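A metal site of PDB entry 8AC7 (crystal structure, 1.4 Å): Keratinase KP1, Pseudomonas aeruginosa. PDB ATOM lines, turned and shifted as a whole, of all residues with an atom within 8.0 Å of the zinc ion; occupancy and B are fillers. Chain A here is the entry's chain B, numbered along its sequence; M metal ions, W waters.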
ATOM      1  N   ILE A 354       3.564 -24.838 -11.164  1.00  0.00           N
ATOM      2  CA  ILE A 354       3.038 -23.479 -11.205  1.00  0.00           C
ATOM      3  C   ILE A 354       2.670 -23.095  -9.779  1.00  0.00           C
ATOM      4  O   ILE A 354       1.993 -23.858  -9.084  1.00  0.00           O
ATOM      5  CB  ILE A 354       1.808 -23.392 -12.133  1.00  0.00           C
ATOM      6  CG1 ILE A 354       2.196 -23.746 -13.568  1.00  0.00           C
ATOM      7  CG2 ILE A 354       1.162 -22.005 -12.040  1.00  0.00           C
ATOM      8  CD1 ILE A 354       0.997 -23.926 -14.504  1.00  0.00           C
ATOM      9  N   TYR A 355       3.091 -21.906  -9.339  1.00  0.00           N
ATOM     10  CA  TYR A 355       2.781 -21.482  -7.983  1.00  0.00           C
ATOM     11  C   TYR A 355       1.278 -21.579  -7.731  1.00  0.00           C
ATOM     12  O   TYR A 355       0.467 -21.114  -8.529  1.00  0.00           O
ATOM     13  CB  TYR A 355       3.227 -20.034  -7.761  1.00  0.00           C
ATOM     14  CG  TYR A 355       4.725 -19.787  -7.671  1.00  0.00           C
ATOM     15  CD1 TYR A 355       5.202 -18.521  -7.363  1.00  0.00           C
ATOM     16  CD2 TYR A 355       5.658 -20.800  -7.896  1.00  0.00           C
ATOM     17  CE1 TYR A 355       6.530 -18.261  -7.284  1.00  0.00           C
ATOM     18  CE2 TYR A 355       7.016 -20.541  -7.809  1.00  0.00           C
ATOM     19  CZ  TYR A 355       7.435 -19.265  -7.509  1.00  0.00           C
ATOM     20  OH  TYR A 355       8.780 -18.963  -7.418  1.00  0.00           O
ATOM     21  N   ASP A 356       0.915 -22.166  -6.585  1.00  0.00           N
ATOM     22  CA  ASP A 356      -0.488 -22.441  -6.251  1.00  0.00           C
ATOM     23  C   ASP A 356      -1.151 -21.226  -5.593  1.00  0.00           C
ATOM     24  O   ASP A 356      -1.581 -21.245  -4.443  1.00  0.00           O
ATOM     25  CB  ASP A 356      -0.535 -23.674  -5.338  1.00  0.00           C
ATOM     26  CG  ASP A 356      -1.938 -24.071  -4.958  1.00  0.00           C
ATOM     27  OD1 ASP A 356      -2.859 -23.960  -5.781  1.00  0.00           O
ATOM     28  OD2 ASP A 356      -2.122 -24.548  -3.818  1.00  0.00           O
ATOM     29  N   GLY A 357      -1.255 -20.139  -6.376  1.00  0.00           N
ATOM     30  CA  GLY A 357      -1.769 -18.882  -5.853  1.00  0.00           C
ATOM     31  C   GLY A 357      -3.199 -18.930  -5.359  1.00  0.00           C
ATOM     32  O   GLY A 357      -3.609 -18.112  -4.528  1.00  0.00           O
ATOM     33  N   ASP A 358      -4.007 -19.858  -5.881  1.00  0.00           N
ATOM     34  CA  ASP A 358      -5.392 -20.000  -5.449  1.00  0.00           C
ATOM     35  C   ASP A 358      -5.552 -20.964  -4.272  1.00  0.00           C
ATOM     36  O   ASP A 358      -6.683 -21.193  -3.840  1.00  0.00           O
ATOM     37  CB  ASP A 358      -6.312 -20.419  -6.604  1.00  0.00           C
ATOM     38  CG  ASP A 358      -5.974 -21.773  -7.202  1.00  0.00           C
ATOM     39  OD1 ASP A 358      -5.076 -22.477  -6.677  1.00  0.00           O
ATOM     40  OD2 ASP A 358      -6.613 -22.149  -8.206  1.00  0.00           O
ATOM     41  N   GLY A 359      -4.459 -21.519  -3.757  1.00  0.00           N
ATOM     42  CA  GLY A 359      -4.559 -22.439  -2.634  1.00  0.00           C
ATOM     43  C   GLY A 359      -5.246 -23.760  -2.927  1.00  0.00           C
ATOM     44  O   GLY A 359      -5.573 -24.486  -1.987  1.00  0.00           O
ATOM     45  N   SER A 360      -5.473 -24.085  -4.208  1.00  0.00           N
ATOM     46  CA  SER A 360      -6.221 -25.283  -4.563  1.00  0.00           C
ATOM     47  C   SER A 360      -5.544 -26.568  -4.081  1.00  0.00           C
ATOM     48  O   SER A 360      -6.226 -27.559  -3.805  1.00  0.00           O
ATOM     49  CB  SER A 360      -6.427 -25.339  -6.082  1.00  0.00           C
ATOM     50  OG  SER A 360      -5.180 -25.430  -6.778  1.00  0.00           O
ATOM     51  N   ASP A 361      -4.211 -26.568  -3.985  1.00  0.00           N
ATOM     52  CA  ASP A 361      -3.461 -27.755  -3.587  1.00  0.00           C
ATOM     53  C   ASP A 361      -3.054 -27.742  -2.126  1.00  0.00           C
ATOM     54  O   ASP A 361      -3.200 -28.759  -1.434  1.00  0.00           O
ATOM     55  CB  ASP A 361      -2.194 -27.895  -4.436  1.00  0.00           C
ATOM     56  CG  ASP A 361      -2.492 -28.112  -5.912  1.00  0.00           C
ATOM     57  OD1 ASP A 361      -3.320 -28.975  -6.244  1.00  0.00           O
ATOM     58  OD2 ASP A 361      -1.888 -27.388  -6.738  1.00  0.00           O
ATOM     59  N   PHE A 362      -2.550 -26.617  -1.634  1.00  0.00           N
ATOM     60  CA  PHE A 362      -1.927 -26.562  -0.329  1.00  0.00           C
ATOM     61  C   PHE A 362      -2.611 -25.625   0.665  1.00  0.00           C
ATOM     62  O   PHE A 362      -2.120 -25.483   1.794  1.00  0.00           O
ATOM     63  CB  PHE A 362      -0.430 -26.237  -0.465  1.00  0.00           C
ATOM     64  CG  PHE A 362       0.262 -27.053  -1.517  1.00  0.00           C
ATOM     65  CD1 PHE A 362       0.600 -26.485  -2.739  1.00  0.00           C
ATOM     66  CD2 PHE A 362       0.549 -28.395  -1.307  1.00  0.00           C
ATOM     67  CE1 PHE A 362       1.227 -27.239  -3.719  1.00  0.00           C
ATOM     68  CE2 PHE A 362       1.174 -29.155  -2.279  1.00  0.00           C
ATOM     69  CZ  PHE A 362       1.514 -28.564  -3.495  1.00  0.00           C
ATOM     70  N   GLY A 363      -3.721 -24.991   0.301  1.00  0.00           N
ATOM     71  CA  GLY A 363      -4.514 -24.210   1.230  1.00  0.00           C
ATOM     72  C   GLY A 363      -3.991 -22.828   1.566  1.00  0.00           C
ATOM     73  O   GLY A 363      -4.617 -22.133   2.368  1.00  0.00           O
ATOM     74  N   LEU A 364      -2.878 -22.397   0.988  1.00  0.00           N
ATOM     75  CA  LEU A 364      -2.348 -21.062   1.196  1.00  0.00           C
ATOM     76  C   LEU A 364      -2.617 -20.239  -0.056  1.00  0.00           C
ATOM     77  O   LEU A 364      -2.159 -20.598  -1.147  1.00  0.00           O
ATOM     78  CB  LEU A 364      -0.844 -21.110   1.484  1.00  0.00           C
ATOM     79  CG  LEU A 364      -0.144 -19.772   1.741  1.00  0.00           C
ATOM     80  CD1 LEU A 364      -0.780 -19.019   2.902  1.00  0.00           C
ATOM     81  CD2 LEU A 364       1.345 -19.971   1.982  1.00  0.00           C
ATOM     82  N   SER A 370      -3.640 -13.266  -7.484  1.00  0.00           N
ATOM     83  CA  SER A 370      -2.727 -14.394  -7.610  1.00  0.00           C
ATOM     84  C   SER A 370      -3.406 -15.581  -8.292  1.00  0.00           C
ATOM     85  O   SER A 370      -2.756 -16.315  -9.053  1.00  0.00           O
ATOM     86  CB  SER A 370      -2.227 -14.797  -6.220  1.00  0.00           C
ATOM     87  OG  SER A 370      -1.510 -13.741  -5.608  1.00  0.00           O
ATOM     88  N   ALA A 371      -4.694 -15.788  -8.042  1.00  0.00           N
ATOM     89  CA  ALA A 371      -5.394 -16.875  -8.714  1.00  0.00           C
ATOM     90  C   ALA A 371      -5.440 -16.659 -10.220  1.00  0.00           C
ATOM     91  O   ALA A 371      -5.210 -17.593 -10.996  1.00  0.00           O
ATOM     92  CB  ALA A 371      -6.799 -17.041  -8.137  1.00  0.00           C
ATOM     93  N   GLU A 374      -1.995 -17.522 -11.737  1.00  0.00           N
ATOM     94  CA  GLU A 374      -1.867 -18.973 -11.815  1.00  0.00           C
ATOM     95  C   GLU A 374      -2.676 -19.535 -12.976  1.00  0.00           C
ATOM     96  O   GLU A 374      -2.194 -20.410 -13.714  1.00  0.00           O
ATOM     97  CB  GLU A 374      -2.329 -19.576 -10.486  1.00  0.00           C
ATOM     98  CG  GLU A 374      -2.288 -21.090 -10.403  1.00  0.00           C
ATOM     99  CD  GLU A 374      -2.915 -21.605  -9.115  1.00  0.00           C
ATOM    100  OE1 GLU A 374      -3.636 -20.827  -8.469  1.00  0.00           O
ATOM    101  OE2 GLU A 374      -2.689 -22.788  -8.754  1.00  0.00           O
ATOM    102  N   ARG A 375      -3.902 -19.041 -13.144  1.00  0.00           N
ATOM    103  CA  ARG A 375      -4.781 -19.542 -14.196  1.00  0.00           C
ATOM    104  C   ARG A 375      -4.193 -19.251 -15.583  1.00  0.00           C
ATOM    105  O   ARG A 375      -4.316 -20.083 -16.494  1.00  0.00           O
ATOM    106  CB  ARG A 375      -6.163 -18.912 -14.036  1.00  0.00           C
ATOM    107  CG  ARG A 375      -7.259 -19.559 -14.873  1.00  0.00           C
ATOM    108  CD  ARG A 375      -8.635 -19.058 -14.421  1.00  0.00           C
ATOM    109  NE  ARG A 375      -8.874 -19.334 -13.004  1.00  0.00           N
ATOM    110  CZ  ARG A 375      -8.960 -18.398 -12.055  1.00  0.00           C
ATOM    111  NH1 ARG A 375      -8.821 -17.121 -12.369  1.00  0.00           N
ATOM    112  NH2 ARG A 375      -9.192 -18.756 -10.793  1.00  0.00           N
ATOM    113  N   GLU A 378      -1.531 -21.861 -16.043  1.00  0.00           N
ATOM    114  CA  GLU A 378      -2.173 -23.151 -16.259  1.00  0.00           C
ATOM    115  C   GLU A 378      -2.743 -23.254 -17.667  1.00  0.00           C
ATOM    116  O   GLU A 378      -2.574 -24.273 -18.345  1.00  0.00           O
ATOM    117  CB  GLU A 378      -3.292 -23.366 -15.235  1.00  0.00           C
ATOM    118  CG  GLU A 378      -2.793 -23.579 -13.811  1.00  0.00           C
ATOM    119  CD  GLU A 378      -3.915 -23.551 -12.776  1.00  0.00           C
ATOM    120  OE1 GLU A 378      -3.699 -24.035 -11.648  1.00  0.00           O
ATOM    121  OE2 GLU A 378      -5.018 -23.043 -13.082  1.00  0.00           O
ATOM    122  N   GLU A 389       1.146 -28.856 -12.474  1.00  0.00           N
ATOM    123  CA  GLU A 389       0.549 -29.044 -11.151  1.00  0.00           C
ATOM    124  C   GLU A 389       1.068 -27.959 -10.229  1.00  0.00           C
ATOM    125  O   GLU A 389       2.020 -27.246 -10.546  1.00  0.00           O
ATOM    126  CB  GLU A 389       0.845 -30.436 -10.584  1.00  0.00           C
ATOM    127  CG  GLU A 389       2.312 -30.661 -10.239  1.00  0.00           C
ATOM    128  CD  GLU A 389       2.596 -32.130 -10.000  1.00  0.00           C
ATOM    129  OE1 GLU A 389       2.700 -32.881 -10.993  1.00  0.00           O
ATOM    130  OE2 GLU A 389       2.695 -32.529  -8.823  1.00  0.00           O
ATOM    131  N   GLY A 390       0.423 -27.832  -9.073  1.00  0.00           N
ATOM    132  CA  GLY A 390       0.767 -26.783  -8.150  1.00  0.00           C
ATOM    133  C   GLY A 390       2.035 -27.053  -7.359  1.00  0.00           C
ATOM    134  O   GLY A 390       2.477 -28.192  -7.178  1.00  0.00           O
ATOM    135  N   THR A 391       2.644 -25.967  -6.895  1.00  0.00           N
ATOM    136  CA  THR A 391       3.741 -26.048  -5.934  1.00  0.00           C
ATOM    137  C   THR A 391       3.499 -25.002  -4.848  1.00  0.00           C
ATOM    138  O   THR A 391       2.790 -24.017  -5.056  1.00  0.00           O
ATOM    139  CB  THR A 391       5.102 -25.867  -6.617  1.00  0.00           C
ATOM    140  OG1 THR A 391       6.152 -26.237  -5.704  1.00  0.00           O
ATOM    141  CG2 THR A 391       5.316 -24.427  -7.056  1.00  0.00           C
HETATM  142 ZN    ZN M   1      -3.890 -23.927  -7.563  1.00  0.00          ZN
HETATM  143  O   HOH W   1      -2.847 -25.563  -8.269  1.00  0.00           O
HETATM  144  O   HOH W   2      -5.234 -24.031  -9.357  1.00  0.00           O
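The zinc ion is bound by the side-chain carboxylate (OE2) of Glu 374 (2.0 Å), the side-chain carboxylate (OD1) of Asp 356 (2.1 Å), water W1 (2.1 Å), the side-chain carboxylate (OD1) of Asp 358 (2.1 Å), the side-chain hydroxyl (OG) of Ser 360 (2.1 Å) and water W2 (2.2 Å).
The backbone NH of Asp 356 is in hydrogen-bond range of the backbone carbonyl oxygen of Thr 391, 3.0 Å away. The backbone NH (N) of Asp 361 is in hydrogen-bond range of the side-chain carboxylate (OD2) of Asp 356, at 2.9 Å. N of Gly 357 lies within hydrogen-bond range of OE1 of Glu 374 (3.2 Å). OD2 of Asp 356 lies within hydrogen-bond range of N of Phe 362.
Water W2 bridges the side-chain carboxylate of Asp 358 (2.6 Å) and the side-chain carboxylate of Glu 378 (2.8 Å).
Within 4 Å of the zinc ion: Asp 356, Asp 358, Ser 360 and Glu 374.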
